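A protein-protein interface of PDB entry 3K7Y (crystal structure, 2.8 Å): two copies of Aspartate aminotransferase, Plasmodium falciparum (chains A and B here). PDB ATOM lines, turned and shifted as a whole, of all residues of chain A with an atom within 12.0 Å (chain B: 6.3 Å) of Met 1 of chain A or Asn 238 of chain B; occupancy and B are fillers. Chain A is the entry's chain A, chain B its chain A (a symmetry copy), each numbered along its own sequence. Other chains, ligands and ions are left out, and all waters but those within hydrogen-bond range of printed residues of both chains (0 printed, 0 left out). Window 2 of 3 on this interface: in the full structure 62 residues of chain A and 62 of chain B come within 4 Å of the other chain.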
ATOM      1  N   MET A   1      11.973  10.840 -28.639  1.00  0.00           N
ATOM      2  CA  MET A   1      10.552  10.447 -28.403  1.00  0.00           C
ATOM      3  C   MET A   1      10.317   9.005 -28.890  1.00  0.00           C
ATOM      4  O   MET A   1      10.337   8.749 -30.108  1.00  0.00           O
ATOM      5  CB  MET A   1       9.607  11.421 -29.134  1.00  0.00           C
ATOM      6  CG  MET A   1       8.477  12.035 -28.282  1.00  0.00           C
ATOM      7  SD  MET A   1       8.936  13.612 -27.475  1.00  0.00           S
ATOM      8  CE  MET A   1       7.326  14.358 -27.125  1.00  0.00           C
ATOM      9  N   ASP A   2      10.117   8.079 -27.939  1.00  0.00           N
ATOM     10  CA  ASP A   2       9.778   6.672 -28.231  1.00  0.00           C
ATOM     11  C   ASP A   2       8.505   6.584 -29.076  1.00  0.00           C
ATOM     12  O   ASP A   2       7.420   7.001 -28.647  1.00  0.00           O
ATOM     13  CB  ASP A   2       9.580   5.850 -26.939  1.00  0.00           C
ATOM     14  CG  ASP A   2      10.887   5.309 -26.353  1.00  0.00           C
ATOM     15  OD1 ASP A   2      11.976   5.744 -26.781  1.00  0.00           O
ATOM     16  OD2 ASP A   2      10.819   4.447 -25.445  1.00  0.00           O
ATOM     17  N   LYS A   3       8.653   6.045 -30.281  1.00  0.00           N
ATOM     18  CA  LYS A   3       7.530   5.812 -31.174  1.00  0.00           C
ATOM     19  C   LYS A   3       7.348   4.313 -31.371  1.00  0.00           C
ATOM     20  O   LYS A   3       6.250   3.862 -31.694  1.00  0.00           O
ATOM     21  CB  LYS A   3       7.764   6.539 -32.509  1.00  0.00           C
ATOM     22  CG  LYS A   3       6.967   6.043 -33.726  1.00  0.00           C
ATOM     23  CD  LYS A   3       7.613   4.817 -34.396  1.00  0.00           C
ATOM     24  CE  LYS A   3       8.947   5.149 -35.058  1.00  0.00           C
ATOM     25  NZ  LYS A   3       9.800   3.941 -35.246  1.00  0.00           N
ATOM     26  N   LEU A   4       8.428   3.557 -31.161  1.00  0.00           N
ATOM     27  CA  LEU A   4       8.465   2.098 -31.344  1.00  0.00           C
ATOM     28  C   LEU A   4       7.176   1.417 -30.918  1.00  0.00           C
ATOM     29  O   LEU A   4       6.715   0.470 -31.572  1.00  0.00           O
ATOM     30  CB  LEU A   4       9.620   1.492 -30.550  1.00  0.00           C
ATOM     31  CG  LEU A   4      10.920   2.286 -30.489  1.00  0.00           C
ATOM     32  CD1 LEU A   4      11.890   1.589 -29.558  1.00  0.00           C
ATOM     33  CD2 LEU A   4      11.516   2.466 -31.880  1.00  0.00           C
ATOM     34  N   LEU A   5       6.601   1.932 -29.832  1.00  0.00           N
ATOM     35  CA  LEU A   5       5.375   1.420 -29.220  1.00  0.00           C
ATOM     36  C   LEU A   5       4.128   1.586 -30.114  1.00  0.00           C
ATOM     37  O   LEU A   5       3.000   1.307 -29.692  1.00  0.00           O
ATOM     38  CB  LEU A   5       5.188   2.082 -27.846  1.00  0.00           C
ATOM     39  CG  LEU A   5       6.484   2.332 -27.057  1.00  0.00           C
ATOM     40  CD1 LEU A   5       6.227   2.963 -25.706  1.00  0.00           C
ATOM     41  CD2 LEU A   5       7.308   1.069 -26.879  1.00  0.00           C
ATOM     42  N   SER A   6       4.345   2.027 -31.351  1.00  0.00           N
ATOM     43  CA  SER A   6       3.273   2.142 -32.330  1.00  0.00           C
ATOM     44  C   SER A   6       2.780   0.768 -32.788  1.00  0.00           C
ATOM     45  O   SER A   6       1.576   0.527 -32.801  1.00  0.00           O
ATOM     46  CB  SER A   6       3.673   3.047 -33.508  1.00  0.00           C
ATOM     47  OG  SER A   6       5.016   2.830 -33.905  1.00  0.00           O
ATOM     48  N   SER A   7       3.694  -0.141 -33.126  1.00  0.00           N
ATOM     49  CA  SER A   7       3.282  -1.494 -33.542  1.00  0.00           C
ATOM     50  C   SER A   7       2.932  -2.423 -32.355  1.00  0.00           C
ATOM     51  O   SER A   7       2.779  -3.637 -32.530  1.00  0.00           O
ATOM     52  CB  SER A   7       4.333  -2.133 -34.469  1.00  0.00           C
ATOM     53  OG  SER A   7       5.529  -2.437 -33.769  1.00  0.00           O
ATOM     54  N   LYS B  91       7.100  14.755 -12.963  1.00  0.00           N
ATOM     55  CA  LYS B  91       5.958  14.812 -13.892  1.00  0.00           C
ATOM     56  C   LYS B  91       5.560  13.389 -14.334  1.00  0.00           C
ATOM     57  O   LYS B  91       4.396  13.118 -14.617  1.00  0.00           O
ATOM     58  CB  LYS B  91       6.327  15.647 -15.136  1.00  0.00           C
ATOM     59  CG  LYS B  91       6.442  17.167 -14.943  1.00  0.00           C
ATOM     60  CD  LYS B  91       5.102  17.871 -15.186  1.00  0.00           C
ATOM     61  CE  LYS B  91       5.274  19.266 -15.797  1.00  0.00           C
ATOM     62  NZ  LYS B  91       5.722  20.295 -14.823  1.00  0.00           N
ATOM     63  N   TYR B  92       6.550  12.496 -14.385  1.00  0.00           N
ATOM     64  CA  TYR B  92       6.397  11.137 -14.886  1.00  0.00           C
ATOM     65  C   TYR B  92       5.882  10.147 -13.847  1.00  0.00           C
ATOM     66  O   TYR B  92       5.023   9.330 -14.153  1.00  0.00           O
ATOM     67  CB  TYR B  92       7.731  10.619 -15.424  1.00  0.00           C
ATOM     68  CG  TYR B  92       8.167  11.142 -16.782  1.00  0.00           C
ATOM     69  CD1 TYR B  92       9.490  10.975 -17.214  1.00  0.00           C
ATOM     70  CD2 TYR B  92       7.275  11.786 -17.641  1.00  0.00           C
ATOM     71  CE1 TYR B  92       9.909  11.435 -18.465  1.00  0.00           C
ATOM     72  CE2 TYR B  92       7.686  12.250 -18.899  1.00  0.00           C
ATOM     73  CZ  TYR B  92       9.004  12.071 -19.299  1.00  0.00           C
ATOM     74  OH  TYR B  92       9.416  12.520 -20.529  1.00  0.00           O
ATOM     75  N   LYS B  97       3.399   7.196 -15.642  1.00  0.00           N
ATOM     76  CA  LYS B  97       3.897   7.150 -17.014  1.00  0.00           C
ATOM     77  C   LYS B  97       5.113   6.231 -17.159  1.00  0.00           C
ATOM     78  O   LYS B  97       5.499   5.878 -18.275  1.00  0.00           O
ATOM     79  CB  LYS B  97       4.185   8.562 -17.558  1.00  0.00           C
ATOM     80  CG  LYS B  97       2.944   9.474 -17.700  1.00  0.00           C
ATOM     81  CD  LYS B  97       2.877  10.215 -19.056  1.00  0.00           C
ATOM     82  CE  LYS B  97       4.180  10.940 -19.419  1.00  0.00           C
ATOM     83  NZ  LYS B  97       4.306  11.248 -20.880  1.00  0.00           N
ATOM     84  N   VAL B 203      18.579  15.392 -29.712  1.00  0.00           N
ATOM     85  CA  VAL B 203      17.708  14.253 -29.439  1.00  0.00           C
ATOM     86  C   VAL B 203      16.261  14.560 -29.805  1.00  0.00           C
ATOM     87  O   VAL B 203      15.549  13.673 -30.265  1.00  0.00           O
ATOM     88  CB  VAL B 203      17.811  13.806 -27.957  1.00  0.00           C
ATOM     89  CG1 VAL B 203      16.751  12.755 -27.611  1.00  0.00           C
ATOM     90  CG2 VAL B 203      19.194  13.273 -27.671  1.00  0.00           C
ATOM     91  N   LEU B 204      15.840  15.809 -29.611  1.00  0.00           N
ATOM     92  CA  LEU B 204      14.495  16.244 -30.000  1.00  0.00           C
ATOM     93  C   LEU B 204      14.300  16.334 -31.514  1.00  0.00           C
ATOM     94  O   LEU B 204      13.263  15.914 -32.034  1.00  0.00           O
ATOM     95  CB  LEU B 204      14.151  17.587 -29.362  1.00  0.00           C
ATOM     96  CG  LEU B 204      13.680  17.528 -27.914  1.00  0.00           C
ATOM     97  CD1 LEU B 204      13.863  18.885 -27.255  1.00  0.00           C
ATOM     98  CD2 LEU B 204      12.237  17.067 -27.829  1.00  0.00           C
ATOM     99  N   LYS B 207      14.672  12.720 -32.851  1.00  0.00           N
ATOM    100  CA  LYS B 207      13.709  11.835 -32.186  1.00  0.00           C
ATOM    101  C   LYS B 207      14.309  10.492 -31.727  1.00  0.00           C
ATOM    102  O   LYS B 207      13.578   9.529 -31.474  1.00  0.00           O
ATOM    103  CB  LYS B 207      12.466  11.642 -33.069  1.00  0.00           C
ATOM    104  CG  LYS B 207      11.717  12.947 -33.399  1.00  0.00           C
ATOM    105  CD  LYS B 207      10.910  12.855 -34.702  1.00  0.00           C
ATOM    106  CE  LYS B 207      11.808  12.975 -35.952  1.00  0.00           C
ATOM    107  NZ  LYS B 207      11.162  12.543 -37.250  1.00  0.00           N
ATOM    108  N   HIS B 208      15.633  10.450 -31.592  1.00  0.00           N
ATOM    109  CA  HIS B 208      16.347   9.256 -31.140  1.00  0.00           C
ATOM    110  C   HIS B 208      15.708   8.593 -29.930  1.00  0.00           C
ATOM    111  O   HIS B 208      15.002   9.233 -29.150  1.00  0.00           O
ATOM    112  CB  HIS B 208      17.793   9.588 -30.789  1.00  0.00           C
ATOM    113  CG  HIS B 208      18.659   9.882 -31.969  1.00  0.00           C
ATOM    114  ND1 HIS B 208      19.696  10.786 -31.917  1.00  0.00           N
ATOM    115  CD2 HIS B 208      18.651   9.391 -33.229  1.00  0.00           C
ATOM    116  CE1 HIS B 208      20.297  10.833 -33.093  1.00  0.00           C
ATOM    117  NE2 HIS B 208      19.678   9.999 -33.909  1.00  0.00           N
ATOM    118  N   VAL B 209      15.977   7.302 -29.786  1.00  0.00           N
ATOM    119  CA  VAL B 209      15.512   6.539 -28.649  1.00  0.00           C
ATOM    120  C   VAL B 209      16.705   6.232 -27.769  1.00  0.00           C
ATOM    121  O   VAL B 209      17.648   5.547 -28.201  1.00  0.00           O
ATOM    122  CB  VAL B 209      14.855   5.242 -29.095  1.00  0.00           C
ATOM    123  CG1 VAL B 209      14.621   4.318 -27.897  1.00  0.00           C
ATOM    124  CG2 VAL B 209      13.551   5.553 -29.823  1.00  0.00           C
ATOM    125  N   LYS B 233      16.865  16.459 -16.535  1.00  0.00           N
ATOM    126  CA  LYS B 233      16.726  17.500 -17.533  1.00  0.00           C
ATOM    127  C   LYS B 233      15.884  16.986 -18.712  1.00  0.00           C
ATOM    128  O   LYS B 233      14.898  17.620 -19.072  1.00  0.00           O
ATOM    129  CB  LYS B 233      18.095  18.033 -17.959  1.00  0.00           C
ATOM    130  CG  LYS B 233      18.066  19.512 -18.248  1.00  0.00           C
ATOM    131  CD  LYS B 233      19.391  20.222 -17.941  1.00  0.00           C
ATOM    132  CE  LYS B 233      19.310  21.673 -18.445  1.00  0.00           C
ATOM    133  NZ  LYS B 233      20.539  22.499 -18.246  1.00  0.00           N
ATOM    134  N   PHE B 234      16.254  15.826 -19.270  1.00  0.00           N
ATOM    135  CA  PHE B 234      15.456  15.110 -20.282  1.00  0.00           C
ATOM    136  C   PHE B 234      13.967  15.047 -19.947  1.00  0.00           C
ATOM    137  O   PHE B 234      13.112  15.266 -20.805  1.00  0.00           O
ATOM    138  CB  PHE B 234      15.937  13.668 -20.406  1.00  0.00           C
ATOM    139  CG  PHE B 234      16.794  13.398 -21.601  1.00  0.00           C
ATOM    140  CD1 PHE B 234      18.173  13.546 -21.540  1.00  0.00           C
ATOM    141  CD2 PHE B 234      16.230  12.935 -22.777  1.00  0.00           C
ATOM    142  CE1 PHE B 234      18.972  13.269 -22.648  1.00  0.00           C
ATOM    143  CE2 PHE B 234      17.027  12.663 -23.883  1.00  0.00           C
ATOM    144  CZ  PHE B 234      18.397  12.834 -23.814  1.00  0.00           C
ATOM    145  N   GLU B 235      13.668  14.709 -18.696  1.00  0.00           N
ATOM    146  CA  GLU B 235      12.293  14.595 -18.232  1.00  0.00           C
ATOM    147  C   GLU B 235      11.528  15.915 -18.354  1.00  0.00           C
ATOM    148  O   GLU B 235      10.414  15.949 -18.879  1.00  0.00           O
ATOM    149  CB  GLU B 235      12.258  14.090 -16.796  1.00  0.00           C
ATOM    150  CG  GLU B 235      10.894  14.238 -16.142  1.00  0.00           C
ATOM    151  CD  GLU B 235      10.822  13.550 -14.804  1.00  0.00           C
ATOM    152  OE1 GLU B 235      11.782  13.668 -14.004  1.00  0.00           O
ATOM    153  OE2 GLU B 235       9.801  12.884 -14.560  1.00  0.00           O
ATOM    154  N   GLU B 236      12.116  16.999 -17.860  1.00  0.00           N
ATOM    155  CA  GLU B 236      11.549  18.311 -18.112  1.00  0.00           C
ATOM    156  C   GLU B 236      11.540  18.511 -19.621  1.00  0.00           C
ATOM    157  O   GLU B 236      12.472  18.092 -20.302  1.00  0.00           O
ATOM    158  CB  GLU B 236      12.363  19.398 -17.424  1.00  0.00           C
ATOM    159  CG  GLU B 236      11.683  20.759 -17.450  1.00  0.00           C
ATOM    160  CD  GLU B 236      12.117  21.650 -16.305  1.00  0.00           C
ATOM    161  OE1 GLU B 236      13.304  21.559 -15.912  1.00  0.00           O
ATOM    162  OE2 GLU B 236      11.276  22.434 -15.797  1.00  0.00           O
ATOM    163  N   LYS B 237      10.493  19.147 -20.144  1.00  0.00           N
ATOM    164  CA  LYS B 237      10.198  19.109 -21.584  1.00  0.00           C
ATOM    165  C   LYS B 237      10.274  17.653 -22.055  1.00  0.00           C
ATOM    166  O   LYS B 237      11.218  17.233 -22.717  1.00  0.00           O
ATOM    167  CB  LYS B 237      11.085  20.075 -22.396  1.00  0.00           C
ATOM    168  CG  LYS B 237      10.423  21.465 -22.673  1.00  0.00           C
ATOM    169  CD  LYS B 237      10.533  22.465 -21.493  1.00  0.00           C
ATOM    170  CE  LYS B 237       9.384  23.493 -21.462  1.00  0.00           C
ATOM    171  NZ  LYS B 237       9.316  24.402 -22.643  1.00  0.00           N
ATOM    172  N   ASN B 238       9.236  16.914 -21.684  1.00  0.00           N
ATOM    173  CA  ASN B 238       9.253  15.467 -21.656  1.00  0.00           C
ATOM    174  C   ASN B 238       9.646  14.754 -22.931  1.00  0.00           C
ATOM    175  O   ASN B 238       8.995  14.896 -23.960  1.00  0.00           O
ATOM    176  CB  ASN B 238       7.923  14.917 -21.117  1.00  0.00           C
ATOM    177  CG  ASN B 238       6.712  15.478 -21.825  1.00  0.00           C
ATOM    178  OD1 ASN B 238       6.718  15.706 -23.034  1.00  0.00           O
ATOM    179  ND2 ASN B 238       5.653  15.690 -21.067  1.00  0.00           N
ATOM    180  N   ILE B 239      10.731  13.992 -22.846  1.00  0.00           N
ATOM    181  CA  ILE B 239      11.136  13.073 -23.904  1.00  0.00           C
ATOM    182  C   ILE B 239      11.019  11.666 -23.317  1.00  0.00           C
ATOM    183  O   ILE B 239      11.068  11.502 -22.091  1.00  0.00           O
ATOM    184  CB  ILE B 239      12.595  13.331 -24.403  1.00  0.00           C
ATOM    185  CG1 ILE B 239      12.939  14.827 -24.417  1.00  0.00           C
ATOM    186  CG2 ILE B 239      12.792  12.728 -25.797  1.00  0.00           C
ATOM    187  CD1 ILE B 239      14.397  15.144 -24.726  1.00  0.00           C
ATOM    188  N   ALA B 240      10.846  10.660 -24.179  1.00  0.00           N
ATOM    189  CA  ALA B 240      10.745   9.258 -23.741  1.00  0.00           C
ATOM    190  C   ALA B 240      12.079   8.499 -23.878  1.00  0.00           C
ATOM    191  O   ALA B 240      12.886   8.799 -24.764  1.00  0.00           O
ATOM    192  CB  ALA B 240       9.640   8.554 -24.499  1.00  0.00           C
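The backbone NH (N) of Met 1 of chain A lies within hydrogen-bond range of the backbone carbonyl oxygen (O) of His 208 of chain B, 3.5 Å away. The side-chain sulfur (SD) of Met 1 of chain A sits close to the backbone carbonyl oxygen (O) of Asn 238 of chain B.
The backbone NH (N) of Ile 239 of chain B is in hydrogen-bond range of the backbone carbonyl oxygen (O) of Phe 234 of chain B. OH of Tyr 92 of chain B sits at hydrogen-bond distance from O of Ile 239 of chain B, 2.5 Å away. The backbone carbonyl oxygen of Val 203 of chain B is in hydrogen-bond range of the backbone NH of His 208 of chain B (3.5 Å).
N of Met 1 of chain A touches O of Lys 207 of chain B, at 3.5 Å. Ile 239 of chain B touches Met 1 of chain A (CG2 to N, 3.5 Å). OD1 of Asp 2 of chain A touches CG1 of Val 209 of chain B, at 3.2 Å. CB of Ala 240 of chain B touches N of Asp 2 of chain A (3.5 Å).
Of the printed residues of chain B, Met 1 of chain A touches Lys 207, His 208, Asn 238 and Ile 239. Asn 238 of chain B touches one residue of chain A. No residue of chain A comes within 4 Å of Leu 204 of chain B. Ile 239 of chain B touches just one residue of chain A: Met 1 (3.5 Å). Ala 240 of chain B touches just one residue of chain A: Asp 2 (3.5 Å). Of the printed residues of chain B, Asp 2 of chain A touches Val 209 and Ala 240. Of the printed residues of chain A, Lys 207 of chain B touches Met 1.
Of the 16 printed residues of chain B, 6 touch a printed residue of chain A. Hydrophobic or aromatic side chains of chain B that line the printed part of chain A: Val 209, Ile 239 and Ala 240. Along chain B the printed residues that touch a printed residue of chain A span positions 207 to 240. Of the 7 printed residues of chain A, 2 touch a printed residue of chain B. Hydrophobic or aromatic side chains of chain A within 4 Å of the printed part of chain B: Met 1. Among the printed residues, 6 pairs touch across the chains. Among the printed residues, no Asp or Glu carboxylate lies within 4 Å of a Lys or Arg side-chain nitrogen of the other chain.
No position is printed for both chains.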
